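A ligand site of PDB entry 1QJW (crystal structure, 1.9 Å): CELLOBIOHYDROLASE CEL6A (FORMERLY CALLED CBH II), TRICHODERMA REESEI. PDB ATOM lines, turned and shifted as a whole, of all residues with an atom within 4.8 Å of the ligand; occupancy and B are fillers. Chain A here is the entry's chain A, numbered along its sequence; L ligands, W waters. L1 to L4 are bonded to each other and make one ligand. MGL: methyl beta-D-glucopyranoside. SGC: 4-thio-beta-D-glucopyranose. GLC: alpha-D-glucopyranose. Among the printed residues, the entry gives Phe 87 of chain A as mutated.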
ATOM      1  N   TRP A  53      16.421  -3.543  20.128  1.00  0.00           N
ATOM      2  CA  TRP A  53      16.761  -3.420  18.716  1.00  0.00           C
ATOM      3  C   TRP A  53      17.927  -4.298  18.268  1.00  0.00           C
ATOM      4  O   TRP A  53      18.986  -4.300  18.876  1.00  0.00           O
ATOM      5  CB  TRP A  53      17.084  -1.970  18.369  1.00  0.00           C
ATOM      6  CG  TRP A  53      15.919  -1.033  18.491  1.00  0.00           C
ATOM      7  CD1 TRP A  53      15.183  -0.782  19.605  1.00  0.00           C
ATOM      8  CD2 TRP A  53      15.387  -0.193  17.461  1.00  0.00           C
ATOM      9  NE1 TRP A  53      14.219   0.174  19.340  1.00  0.00           N
ATOM     10  CE2 TRP A  53      14.323   0.554  18.026  1.00  0.00           C
ATOM     11  CE3 TRP A  53      15.715   0.022  16.105  1.00  0.00           C
ATOM     12  CZ2 TRP A  53      13.576   1.472  17.296  1.00  0.00           C
ATOM     13  CZ3 TRP A  53      14.969   0.940  15.375  1.00  0.00           C
ATOM     14  CH2 TRP A  53      13.913   1.656  15.973  1.00  0.00           C
ATOM     15  N   ASP A  55      19.960  -3.985  15.818  1.00  0.00           N
ATOM     16  CA  ASP A  55      20.531  -3.067  14.826  1.00  0.00           C
ATOM     17  C   ASP A  55      21.847  -3.517  14.190  1.00  0.00           C
ATOM     18  O   ASP A  55      22.355  -2.858  13.280  1.00  0.00           O
ATOM     19  CB  ASP A  55      20.689  -1.672  15.454  1.00  0.00           C
ATOM     20  CG  ASP A  55      21.659  -1.650  16.621  1.00  0.00           C
ATOM     21  OD1 ASP A  55      21.570  -2.540  17.493  1.00  0.00           O
ATOM     22  OD2 ASP A  55      22.505  -0.734  16.669  1.00  0.00           O
ATOM     23  N   PHE A  87      16.066  -4.528  12.369  1.00  0.00           N
ATOM     24  CA  PHE A  87      16.533  -3.265  11.791  1.00  0.00           C
ATOM     25  C   PHE A  87      17.974  -3.309  11.284  1.00  0.00           C
ATOM     26  O   PHE A  87      18.875  -2.767  11.916  1.00  0.00           O
ATOM     27  CB  PHE A  87      16.389  -2.180  12.872  1.00  0.00           C
ATOM     28  CG  PHE A  87      16.759  -0.779  12.437  1.00  0.00           C
ATOM     29  CD1 PHE A  87      16.064  -0.143  11.415  1.00  0.00           C
ATOM     30  CD2 PHE A  87      17.767  -0.086  13.102  1.00  0.00           C
ATOM     31  CE1 PHE A  87      16.358   1.177  11.067  1.00  0.00           C
ATOM     32  CE2 PHE A  87      18.073   1.239  12.765  1.00  0.00           C
ATOM     33  CZ  PHE A  87      17.367   1.867  11.741  1.00  0.00           C
ATOM     34  N   ARG A  92      20.506   1.211   4.906  1.00  0.00           N
ATOM     35  CA  ARG A  92      19.488   1.541   5.899  1.00  0.00           C
ATOM     36  C   ARG A  92      19.327   3.043   6.065  1.00  0.00           C
ATOM     37  O   ARG A  92      20.265   3.804   5.830  1.00  0.00           O
ATOM     38  CB  ARG A  92      19.907   0.916   7.237  1.00  0.00           C
ATOM     39  CG  ARG A  92      18.830   0.881   8.315  1.00  0.00           C
ATOM     40  CD  ARG A  92      19.347   0.160   9.552  1.00  0.00           C
ATOM     41  NE  ARG A  92      20.422   0.897  10.204  1.00  0.00           N
ATOM     42  CZ  ARG A  92      21.143   0.433  11.227  1.00  0.00           C
ATOM     43  NH1 ARG A  92      20.910  -0.775  11.715  1.00  0.00           N
ATOM     44  NH2 ARG A  92      22.089   1.192  11.757  1.00  0.00           N
ATOM     45  N   ASP A  93      18.128   3.484   6.444  1.00  0.00           N
ATOM     46  CA  ASP A  93      17.860   4.902   6.686  1.00  0.00           C
ATOM     47  C   ASP A  93      18.255   5.741   5.466  1.00  0.00           C
ATOM     48  O   ASP A  93      18.921   6.764   5.591  1.00  0.00           O
ATOM     49  CB  ASP A  93      18.663   5.311   7.929  1.00  0.00           C
ATOM     50  CG  ASP A  93      18.384   6.727   8.399  1.00  0.00           C
ATOM     51  OD1 ASP A  93      17.201   7.130   8.457  1.00  0.00           O
ATOM     52  OD2 ASP A  93      19.355   7.434   8.738  1.00  0.00           O
ATOM     53  N   ALA A  95      16.941   8.009   3.569  1.00  0.00           N
ATOM     54  CA  ALA A  95      16.674   9.443   3.454  1.00  0.00           C
ATOM     55  C   ALA A  95      17.464  10.315   4.434  1.00  0.00           C
ATOM     56  O   ALA A  95      17.477  11.537   4.302  1.00  0.00           O
ATOM     57  CB  ALA A  95      15.174   9.693   3.634  1.00  0.00           C
ATOM     58  N   ALA A  96      18.134   9.688   5.398  1.00  0.00           N
ATOM     59  CA  ALA A  96      18.912  10.418   6.373  1.00  0.00           C
ATOM     60  C   ALA A  96      20.374   9.948   6.386  1.00  0.00           C
ATOM     61  O   ALA A  96      20.790   9.191   5.520  1.00  0.00           O
ATOM     62  CB  ALA A  96      18.290  10.255   7.767  1.00  0.00           C
ATOM     63  N   SER A  99      21.572   7.170  10.937  1.00  0.00           N
ATOM     64  CA  SER A  99      21.501   5.742  11.226  1.00  0.00           C
ATOM     65  C   SER A  99      21.893   4.781  10.103  1.00  0.00           C
ATOM     66  O   SER A  99      21.342   3.687  10.015  1.00  0.00           O
ATOM     67  CB  SER A  99      20.099   5.382  11.731  1.00  0.00           C
ATOM     68  OG  SER A  99      19.866   5.964  13.008  1.00  0.00           O
ATOM     69  N   PRO A 138      11.916  -0.423  10.930  1.00  0.00           N
ATOM     70  CA  PRO A 138      11.404   0.946  11.038  1.00  0.00           C
ATOM     71  C   PRO A 138      12.193   1.824  10.055  1.00  0.00           C
ATOM     72  O   PRO A 138      13.333   1.510   9.712  1.00  0.00           O
ATOM     73  CB  PRO A 138      11.714   1.328  12.484  1.00  0.00           C
ATOM     74  CG  PRO A 138      11.708   0.010  13.211  1.00  0.00           C
ATOM     75  CD  PRO A 138      12.405  -0.906  12.239  1.00  0.00           C
ATOM     76  N   ASP A 139      11.576   2.905   9.588  1.00  0.00           N
ATOM     77  CA  ASP A 139      12.258   3.829   8.705  1.00  0.00           C
ATOM     78  C   ASP A 139      12.777   3.203   7.403  1.00  0.00           C
ATOM     79  O   ASP A 139      13.924   3.423   7.010  1.00  0.00           O
ATOM     80  CB  ASP A 139      13.404   4.475   9.506  1.00  0.00           C
ATOM     81  CG  ASP A 139      14.194   5.510   8.730  1.00  0.00           C
ATOM     82  OD1 ASP A 139      13.591   6.311   7.993  1.00  0.00           O
ATOM     83  OD2 ASP A 139      15.428   5.516   8.887  1.00  0.00           O
ATOM     84  N   ASN A 143      10.056   5.627   3.467  1.00  0.00           N
ATOM     85  CA  ASN A 143      10.932   6.453   2.633  1.00  0.00           C
ATOM     86  C   ASN A 143      10.595   6.315   1.147  1.00  0.00           C
ATOM     87  O   ASN A 143      10.772   7.261   0.367  1.00  0.00           O
ATOM     88  CB  ASN A 143      12.397   6.077   2.857  1.00  0.00           C
ATOM     89  CG  ASN A 143      12.923   6.543   4.190  1.00  0.00           C
ATOM     90  OD1 ASN A 143      12.978   7.741   4.463  1.00  0.00           O
ATOM     91  ND2 ASN A 143      13.320   5.594   5.043  1.00  0.00           N
ATOM     92  N   THR A 146       7.676   8.931   0.123  1.00  0.00           N
ATOM     93  CA  THR A 146       7.964  10.356  -0.012  1.00  0.00           C
ATOM     94  C   THR A 146       9.383  10.753  -0.384  1.00  0.00           C
ATOM     95  O   THR A 146       9.609  11.886  -0.818  1.00  0.00           O
ATOM     96  CB  THR A 146       7.656  11.099   1.299  1.00  0.00           C
ATOM     97  OG1 THR A 146       8.572  10.657   2.308  1.00  0.00           O
ATOM     98  CG2 THR A 146       6.222  10.820   1.754  1.00  0.00           C
ATOM     99  N   ASN A 147      10.341   9.841  -0.252  1.00  0.00           N
ATOM    100  CA  ASN A 147      11.733  10.196  -0.520  1.00  0.00           C
ATOM    101  C   ASN A 147      12.444   9.576  -1.727  1.00  0.00           C
ATOM    102  O   ASN A 147      13.660   9.409  -1.706  1.00  0.00           O
ATOM    103  CB  ASN A 147      12.559   9.948   0.740  1.00  0.00           C
ATOM    104  CG  ASN A 147      11.955  10.596   1.969  1.00  0.00           C
ATOM    105  OD1 ASN A 147      11.394  11.688   1.884  1.00  0.00           O
ATOM    106  ND2 ASN A 147      12.057   9.929   3.116  1.00  0.00           N
ATOM    107  N   HIS A 184       4.529   7.600  10.521  1.00  0.00           N
ATOM    108  CA  HIS A 184       3.644   8.209  11.517  1.00  0.00           C
ATOM    109  C   HIS A 184       2.750   9.289  10.909  1.00  0.00           C
ATOM    110  O   HIS A 184       2.894   9.647   9.742  1.00  0.00           O
ATOM    111  CB  HIS A 184       4.487   8.802  12.661  1.00  0.00           C
ATOM    112  CG  HIS A 184       5.435   9.871  12.226  1.00  0.00           C
ATOM    113  ND1 HIS A 184       5.035  11.168  12.000  1.00  0.00           N
ATOM    114  CD2 HIS A 184       6.771   9.843  11.987  1.00  0.00           C
ATOM    115  CE1 HIS A 184       6.090  11.898  11.638  1.00  0.00           C
ATOM    116  NE2 HIS A 184       7.146  11.111  11.621  1.00  0.00           N
ATOM    117  N   GLY A 186       2.604  12.501  10.912  1.00  0.00           N
ATOM    118  CA  GLY A 186       3.178  13.654  10.238  1.00  0.00           C
ATOM    119  C   GLY A 186       3.967  13.302   8.992  1.00  0.00           C
ATOM    120  O   GLY A 186       4.488  14.185   8.304  1.00  0.00           O
ATOM    121  N   TRP A 187       4.038  12.013   8.700  1.00  0.00           N
ATOM    122  CA  TRP A 187       4.776  11.532   7.548  1.00  0.00           C
ATOM    123  C   TRP A 187       3.807  10.990   6.496  1.00  0.00           C
ATOM    124  O   TRP A 187       3.587  11.620   5.459  1.00  0.00           O
ATOM    125  CB  TRP A 187       5.740  10.419   7.980  1.00  0.00           C
ATOM    126  CG  TRP A 187       6.793  10.054   6.976  1.00  0.00           C
ATOM    127  CD1 TRP A 187       6.839  10.394   5.655  1.00  0.00           C
ATOM    128  CD2 TRP A 187       7.962   9.254   7.229  1.00  0.00           C
ATOM    129  NE1 TRP A 187       7.963   9.851   5.067  1.00  0.00           N
ATOM    130  CE2 TRP A 187       8.661   9.150   6.011  1.00  0.00           C
ATOM    131  CE3 TRP A 187       8.473   8.612   8.362  1.00  0.00           C
ATOM    132  CZ2 TRP A 187       9.859   8.427   5.890  1.00  0.00           C
ATOM    133  CZ3 TRP A 187       9.662   7.887   8.252  1.00  0.00           C
ATOM    134  CH2 TRP A 187      10.333   7.813   7.021  1.00  0.00           C
ATOM    135  N   VAL A 221       7.235   4.980  15.431  1.00  0.00           N
ATOM    136  CA  VAL A 221       8.467   4.377  15.938  1.00  0.00           C
ATOM    137  C   VAL A 221       9.607   5.394  15.915  1.00  0.00           C
ATOM    138  O   VAL A 221       9.926   5.961  14.876  1.00  0.00           O
ATOM    139  CB  VAL A 221       8.905   3.147  15.105  1.00  0.00           C
ATOM    140  CG1 VAL A 221      10.220   2.591  15.662  1.00  0.00           C
ATOM    141  CG2 VAL A 221       7.831   2.082  15.145  1.00  0.00           C
ATOM    142  N   ALA A 222      10.212   5.617  17.079  1.00  0.00           N
ATOM    143  CA  ALA A 222      11.296   6.568  17.237  1.00  0.00           C
ATOM    144  C   ALA A 222      10.828   8.008  17.030  1.00  0.00           C
ATOM    145  O   ALA A 222      11.646   8.925  16.883  1.00  0.00           O
ATOM    146  CB  ALA A 222      12.441   6.253  16.263  1.00  0.00           C
ATOM    147  N   ASN A 223       9.518   8.223  17.006  1.00  0.00           N
ATOM    148  CA  ASN A 223       9.025   9.588  16.863  1.00  0.00           C
ATOM    149  C   ASN A 223       8.328  10.064  18.136  1.00  0.00           C
ATOM    150  O   ASN A 223       8.424   9.422  19.186  1.00  0.00           O
ATOM    151  CB  ASN A 223       8.119   9.758  15.639  1.00  0.00           C
ATOM    152  CG  ASN A 223       8.248  11.151  15.029  1.00  0.00           C
ATOM    153  OD1 ASN A 223       9.173  11.412  14.243  1.00  0.00           O
ATOM    154  ND2 ASN A 223       7.350  12.045  15.385  1.00  0.00           N
ATOM    155  N   ARG A 271       8.213   8.469  23.820  1.00  0.00           N
ATOM    156  CA  ARG A 271       8.681   9.846  23.964  1.00  0.00           C
ATOM    157  C   ARG A 271       7.576  10.818  23.565  1.00  0.00           C
ATOM    158  O   ARG A 271       7.841  11.911  23.057  1.00  0.00           O
ATOM    159  CB  ARG A 271       9.939  10.069  23.101  1.00  0.00           C
ATOM    160  CG  ARG A 271      11.112   9.167  23.462  1.00  0.00           C
ATOM    161  CD  ARG A 271      12.408   9.556  22.743  1.00  0.00           C
ATOM    162  NE  ARG A 271      12.357   9.336  21.304  1.00  0.00           N
ATOM    163  CZ  ARG A 271      13.332   9.686  20.467  1.00  0.00           C
ATOM    164  NH1 ARG A 271      14.444  10.259  20.910  1.00  0.00           N
ATOM    165  NH2 ARG A 271      13.190   9.460  19.155  1.00  0.00           N
ATOM    166  N   TRP A 282       7.478  20.180  12.151  1.00  0.00           N
ATOM    167  CA  TRP A 282       7.032  18.807  12.359  1.00  0.00           C
ATOM    168  C   TRP A 282       8.047  17.768  11.866  1.00  0.00           C
ATOM    169  O   TRP A 282       8.166  16.685  12.441  1.00  0.00           O
ATOM    170  CB  TRP A 282       5.695  18.578  11.654  1.00  0.00           C
ATOM    171  CG  TRP A 282       4.860  17.490  12.253  1.00  0.00           C
ATOM    172  CD1 TRP A 282       5.215  16.636  13.257  1.00  0.00           C
ATOM    173  CD2 TRP A 282       3.523  17.138  11.878  1.00  0.00           C
ATOM    174  NE1 TRP A 282       4.173  15.778  13.534  1.00  0.00           N
ATOM    175  CE2 TRP A 282       3.127  16.064  12.698  1.00  0.00           C
ATOM    176  CE3 TRP A 282       2.620  17.627  10.922  1.00  0.00           C
ATOM    177  CZ2 TRP A 282       1.858  15.465  12.597  1.00  0.00           C
ATOM    178  CZ3 TRP A 282       1.362  17.036  10.823  1.00  0.00           C
ATOM    179  CH2 TRP A 282       0.998  15.965  11.652  1.00  0.00           C
ATOM    180  N   GLY A 283       8.767  18.114  10.803  1.00  0.00           N
ATOM    181  CA  GLY A 283       9.747  17.213  10.244  1.00  0.00           C
ATOM    182  C   GLY A 283      11.046  17.084  11.025  1.00  0.00           C
ATOM    183  O   GLY A 283      11.930  16.312  10.649  1.00  0.00           O
ATOM    184  N   TRP A 285      13.017  15.522  13.493  1.00  0.00           N
ATOM    185  CA  TRP A 285      12.976  14.246  14.201  1.00  0.00           C
ATOM    186  C   TRP A 285      14.111  13.932  15.170  1.00  0.00           C
ATOM    187  O   TRP A 285      13.975  13.029  16.000  1.00  0.00           O
ATOM    188  CB  TRP A 285      12.934  13.118  13.170  1.00  0.00           C
ATOM    189  CG  TRP A 285      14.059  13.221  12.169  1.00  0.00           C
ATOM    190  CD1 TRP A 285      14.017  13.854  10.949  1.00  0.00           C
ATOM    191  CD2 TRP A 285      15.399  12.729  12.318  1.00  0.00           C
ATOM    192  NE1 TRP A 285      15.253  13.787  10.343  1.00  0.00           N
ATOM    193  CE2 TRP A 285      16.114  13.100  11.157  1.00  0.00           C
ATOM    194  CE3 TRP A 285      16.068  12.009  13.319  1.00  0.00           C
ATOM    195  CZ2 TRP A 285      17.470  12.784  10.967  1.00  0.00           C
ATOM    196  CZ3 TRP A 285      17.415  11.691  13.140  1.00  0.00           C
ATOM    197  CH2 TRP A 285      18.101  12.081  11.965  1.00  0.00           C
ATOM    198  N   LYS A 313      11.238   2.726  20.473  1.00  0.00           N
ATOM    199  CA  LYS A 313      12.513   3.427  20.578  1.00  0.00           C
ATOM    200  C   LYS A 313      12.748   3.620  22.084  1.00  0.00           C
ATOM    201  O   LYS A 313      11.901   4.182  22.776  1.00  0.00           O
ATOM    202  CB  LYS A 313      12.418   4.795  19.890  1.00  0.00           C
ATOM    203  CG  LYS A 313      13.584   5.744  20.168  1.00  0.00           C
ATOM    204  CD  LYS A 313      14.874   5.259  19.525  1.00  0.00           C
ATOM    205  CE  LYS A 313      16.031   6.202  19.833  1.00  0.00           C
ATOM    206  NZ  LYS A 313      17.242   5.883  19.040  1.00  0.00           N
ATOM    207  N   PRO A 314      13.886   3.124  22.603  1.00  0.00           N
ATOM    208  CA  PRO A 314      14.187   3.260  24.038  1.00  0.00           C
ATOM    209  C   PRO A 314      14.601   4.685  24.404  1.00  0.00           C
ATOM    210  O   PRO A 314      15.650   5.150  23.975  1.00  0.00           O
ATOM    211  CB  PRO A 314      15.322   2.255  24.252  1.00  0.00           C
ATOM    212  CG  PRO A 314      15.183   1.289  23.102  1.00  0.00           C
ATOM    213  CD  PRO A 314      14.849   2.225  21.963  1.00  0.00           C
ATOM    214  N   GLU A 317      18.325   6.539  24.362  1.00  0.00           N
ATOM    215  CA  GLU A 317      19.218   6.169  23.283  1.00  0.00           C
ATOM    216  C   GLU A 317      19.052   7.239  22.201  1.00  0.00           C
ATOM    217  O   GLU A 317      17.945   7.507  21.735  1.00  0.00           O
ATOM    218  CB  GLU A 317      18.885   4.770  22.755  1.00  0.00           C
ATOM    219  CG  GLU A 317      19.013   3.715  23.842  1.00  0.00           C
ATOM    220  CD  GLU A 317      18.790   2.292  23.334  1.00  0.00           C
ATOM    221  OE1 GLU A 317      18.465   2.120  22.148  1.00  0.00           O
ATOM    222  OE2 GLU A 317      18.932   1.354  24.151  1.00  0.00           O
ATOM    223  N   CYS A 318      20.179   7.843  21.834  1.00  0.00           N
ATOM    224  CA  CYS A 318      20.238   8.930  20.859  1.00  0.00           C
ATOM    225  C   CYS A 318      19.726   8.658  19.451  1.00  0.00           C
ATOM    226  O   CYS A 318      19.751   7.521  18.962  1.00  0.00           O
ATOM    227  CB  CYS A 318      21.673   9.446  20.796  1.00  0.00           C
ATOM    228  SG  CYS A 318      21.852  11.082  20.100  1.00  0.00           S
ATOM    229  N   ASP A 319      19.270   9.718  18.784  1.00  0.00           N
ATOM    230  CA  ASP A 319      18.760   9.632  17.423  1.00  0.00           C
ATOM    231  C   ASP A 319      19.846   9.954  16.408  1.00  0.00           C
ATOM    232  O   ASP A 319      19.705   9.656  15.222  1.00  0.00           O
ATOM    233  CB  ASP A 319      17.614  10.629  17.209  1.00  0.00           C
ATOM    234  CG  ASP A 319      16.411  10.351  18.086  1.00  0.00           C
ATOM    235  OD1 ASP A 319      15.982   9.178  18.148  1.00  0.00           O
ATOM    236  OD2 ASP A 319      15.879  11.297  18.696  1.00  0.00           O
ATOM    237  N   ARG A 328      28.321  10.041   9.921  1.00  0.00           N
ATOM    238  CA  ARG A 328      26.873   9.929  10.047  1.00  0.00           C
ATOM    239  C   ARG A 328      26.225  11.214  10.594  1.00  0.00           C
ATOM    240  O   ARG A 328      25.118  11.172  11.125  1.00  0.00           O
ATOM    241  CB  ARG A 328      26.501   8.764  10.966  1.00  0.00           C
ATOM    242  CG  ARG A 328      27.128   7.442  10.586  1.00  0.00           C
ATOM    243  CD  ARG A 328      27.002   6.476  11.750  1.00  0.00           C
ATOM    244  NE  ARG A 328      25.709   5.820  11.812  1.00  0.00           N
ATOM    245  CZ  ARG A 328      25.171   5.316  12.919  1.00  0.00           C
ATOM    246  NH1 ARG A 328      25.825   5.396  14.074  1.00  0.00           N
ATOM    247  NH2 ARG A 328      24.006   4.695  12.879  1.00  0.00           N
ATOM    248  N   ALA A 345      23.951   7.832  17.003  1.00  0.00           N
ATOM    249  CA  ALA A 345      22.618   7.244  17.074  1.00  0.00           C
ATOM    250  C   ALA A 345      22.721   5.935  17.860  1.00  0.00           C
ATOM    251  O   ALA A 345      23.647   5.146  17.643  1.00  0.00           O
ATOM    252  CB  ALA A 345      22.086   6.975  15.668  1.00  0.00           C
ATOM    253  N   GLY A 346      21.770   5.702  18.757  1.00  0.00           N
ATOM    254  CA  GLY A 346      21.767   4.492  19.553  1.00  0.00           C
ATOM    255  C   GLY A 346      22.528   4.585  20.873  1.00  0.00           C
ATOM    256  O   GLY A 346      22.187   3.914  21.844  1.00  0.00           O
HETATM  257  C1  MGL L   1       8.712  13.570   7.750  1.00  0.00           C
HETATM  258  C2  MGL L   1       8.699  12.993   9.164  1.00  0.00           C
HETATM  259  C3  MGL L   1      10.108  12.640   9.633  1.00  0.00           C
HETATM  260  C4  MGL L   1      10.899  11.854   8.576  1.00  0.00           C
HETATM  261  C5  MGL L   1      10.798  12.525   7.203  1.00  0.00           C
HETATM  262  C6  MGL L   1      11.452  11.649   6.140  1.00  0.00           C
HETATM  263  C7  MGL L   1       7.263  14.500   6.076  1.00  0.00           C
HETATM  264  O1  MGL L   1       7.369  13.752   7.295  1.00  0.00           O
HETATM  265  O2  MGL L   1       8.130  13.926  10.061  1.00  0.00           O
HETATM  266  O3  MGL L   1      10.013  11.863  10.814  1.00  0.00           O
HETATM  267  O4  MGL L   1      12.275  11.799   8.959  1.00  0.00           O
HETATM  268  O5  MGL L   1       9.413  12.693   6.870  1.00  0.00           O
HETATM  269  O6  MGL L   1      11.785  12.424   5.009  1.00  0.00           O
HETATM  270  C1  SGC L   2      12.676  10.536   9.473  1.00  0.00           C
HETATM  271  C2  SGC L   2      14.189  10.449   9.510  1.00  0.00           C
HETATM  272  O2  SGC L   2      14.718  10.615   8.213  1.00  0.00           O
HETATM  273  C3  SGC L   2      14.623   9.098  10.103  1.00  0.00           C
HETATM  274  O3  SGC L   2      16.036   9.086  10.247  1.00  0.00           O
HETATM  275  C4  SGC L   2      13.954   8.849  11.457  1.00  0.00           C
HETATM  276  C5  SGC L   2      12.444   9.069  11.341  1.00  0.00           C
HETATM  277  O5  SGC L   2      12.178  10.356  10.805  1.00  0.00           O
HETATM  278  C6  SGC L   2      11.768   8.966  12.702  1.00  0.00           C
HETATM  279  O6  SGC L   2      10.419   9.376  12.595  1.00  0.00           O
HETATM  280  S4  SGC L   2      14.257   7.161  12.064  1.00  0.00           S
HETATM  281  C1  GLC L   3      15.786   7.367  13.022  1.00  0.00           C
HETATM  282  C2  GLC L   3      15.531   7.617  14.515  1.00  0.00           C
HETATM  283  C3  GLC L   3      16.608   6.966  15.411  1.00  0.00           C
HETATM  284  C4  GLC L   3      16.803   5.484  15.135  1.00  0.00           C
HETATM  285  C5  GLC L   3      16.515   5.124  13.672  1.00  0.00           C
HETATM  286  C6  GLC L   3      15.118   4.522  13.505  1.00  0.00           C
HETATM  287  O2  GLC L   3      15.492   9.003  14.769  1.00  0.00           O
HETATM  288  O3  GLC L   3      16.281   7.157  16.768  1.00  0.00           O
HETATM  289  O4  GLC L   3      18.151   5.147  15.457  1.00  0.00           O
HETATM  290  O5  GLC L   3      16.697   6.274  12.821  1.00  0.00           O
HETATM  291  O6  GLC L   3      14.891   4.152  12.161  1.00  0.00           O
HETATM  292  C1  GLC L   4      18.349   3.799  15.908  1.00  0.00           C
HETATM  293  C2  GLC L   4      19.839   3.502  15.923  1.00  0.00           C
HETATM  294  C3  GLC L   4      20.092   2.080  16.425  1.00  0.00           C
HETATM  295  C4  GLC L   4      19.355   1.809  17.746  1.00  0.00           C
HETATM  296  C5  GLC L   4      17.886   2.259  17.686  1.00  0.00           C
HETATM  297  C6  GLC L   4      17.244   2.178  19.062  1.00  0.00           C
HETATM  298  O2  GLC L   4      20.387   3.653  14.632  1.00  0.00           O
HETATM  299  O3  GLC L   4      21.470   1.887  16.606  1.00  0.00           O
HETATM  300  O4  GLC L   4      19.392   0.426  18.030  1.00  0.00           O
HETATM  301  O5  GLC L   4      17.819   3.619  17.222  1.00  0.00           O
HETATM  302  O6  GLC L   4      17.703   3.231  19.887  1.00  0.00           O
HETATM  303  O   HOH W   1      11.566   4.869  12.934  1.00  0.00           O
HETATM  304  O   HOH W   2      18.769   9.359  10.583  1.00  0.00           O
HETATM  305  O   HOH W   3       9.452  14.172  12.735  1.00  0.00           O
HETATM  306  O   HOH W   4      13.320   8.995   6.710  1.00  0.00           O
HETATM  307  O   HOH W   5      15.669   8.040   6.328  1.00  0.00           O
HETATM  308  O   HOH W   6      23.132   3.031  14.481  1.00  0.00           O
HETATM  309  O   HOH W   7      19.493  -0.098  20.754  1.00  0.00           O
HETATM  310  O   HOH W   8       8.556   6.843  12.453  1.00  0.00           O
HETATM  311  O   HOH W   9      18.979   8.284  13.088  1.00  0.00           O
HETATM  312  O   HOH W  10      15.429  13.198   7.403  1.00  0.00           O
HETATM  313  O   HOH W  11      13.258  10.272  15.319  1.00  0.00           O
HETATM  314  O   HOH W  12       6.152  15.752   9.574  1.00  0.00           O
HETATM  315  O   HOH W  13      13.721  14.686   5.854  1.00  0.00           O
HETATM  316  O   HOH W  14      23.419   0.303  14.192  1.00  0.00           O
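OD1 of Asp 319 is in hydrogen-bond range of O3 of GLC L3. The side-chain carboxylate (OE1) of Glu 317 lies within hydrogen-bond range of an oxygen (O6) of GLC L4, 2.6 Å away. The side-chain amino group (NZ) of Lys 313 sits at hydrogen-bond distance from an oxygen (O3) of GLC L3. OD2 of Asp 55 sits at hydrogen-bond distance from O3 of GLC L4. The side-chain hydroxyl of Ser 99 lies within hydrogen-bond range of an oxygen (O2) of GLC L4 (2.9 Å). OD1 of Asp 93 lies within hydrogen-bond range of O3 of SGC L2, at 2.9 Å. The side-chain amide oxygen (OD1) of Asn 223 sits at hydrogen-bond distance from an oxygen (O6) of SGC L2 (2.9 Å). O3 of MGL L1 sits at hydrogen-bond distance from NE2 of His 184. An oxygen (O6) of MGL L1 sits at hydrogen-bond distance from the side-chain amide nitrogen (ND2) of Asn 147 (3.1 Å).
OD2 of Asp 139 lies close to S4 of SGC L2 (3.8 Å). O of Gly 186 lies close to O1 of MGL L1 (3.1 Å). CB of Trp 53 touches O4 of GLC L4, at 3.3 Å. CZ of Phe 87 touches O6 of GLC L3, 3.4 Å away. CB of Ala 96 touches O3 of SGC L2, at 3.5 Å. O of Pro 138 touches O6 of GLC L3 (3.9 Å). Trp 187 touches the ligand. Ala 222 touches the ligand. Trp 282 touches the ligand. Gly 283 touches the ligand. Trp 285 touches the ligand. CD of Pro 314 touches O6 of GLC L4 (3.7 Å). CB of Ala 345 touches O2 of GLC L4 (3.9 Å). CA of Gly 346 touches O3 of GLC L4, 3.9 Å away. Hydrophobic or aromatic side chains that line the ligand: Trp 53, Phe 87, Ala 96, His 184, Trp 187, Ala 222, Trp 285, Pro 314 and Ala 345.
Water W4 lies within hydrogen-bond range of the side-chain amide oxygen (OD1) of Asn 143, an oxygen (O2) of SGC L2 and the side-chain carboxylate (OD1) of Asp 139. Water W11 lies within hydrogen-bond range of the backbone carbonyl oxygen (O) of Ala 222 (2.6 Å), an oxygen (O2) of GLC L3 (2.6 Å) and the backbone carbonyl oxygen (O) of Trp 285 (2.9 Å). Water W2 lies within hydrogen-bond range of the side-chain carboxylate of Asp 93 and an oxygen (O3) of SGC L2. Water W6 lies within hydrogen-bond range of the guanidinium group of Arg 328 (2.5 Å), an oxygen (O2) of GLC L4 (2.8 Å) and the guanidinium group of Arg 92 (3.4 Å). Water W8 bridges the backbone carbonyl oxygen of Val 221 (2.9 Å) and an oxygen (O6) of SGC L2 (3.1 Å). Water W14 lies within hydrogen-bond range of the side-chain carboxylate of Asp 55, the guanidinium group of Arg 92 and an oxygen (O3) of GLC L4.
OD2 of Asp 319 lies within salt-bridge range of NH1 of Arg 271 (2.8 Å). The side-chain amino group of Lys 313 sits close to the backbone carbonyl oxygen of Glu 317 (3.2 Å). The backbone carbonyl oxygen (O) of Cys 318 lies within hydrogen-bond range of the side-chain amino group (NZ) of Lys 313 (3.0 Å). The backbone carbonyl oxygen of Asp 55 lies within hydrogen-bond range of the guanidinium group of Arg 92 (3.0 Å). OD2 of Asp 93 is in hydrogen-bond range of N of Ser 99 (3.1 Å). O of Ser 99 is in hydrogen-bond range of NE of Arg 92 (2.9 Å). A ring nitrogen (ND1) of His 184 lies within hydrogen-bond range of the backbone NH (N) of Gly 186. The side-chain hydroxyl (OG1) of Thr 146 is in hydrogen-bond range of the side-chain amide oxygen (OD1) of Asn 147, at 3.0 Å.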
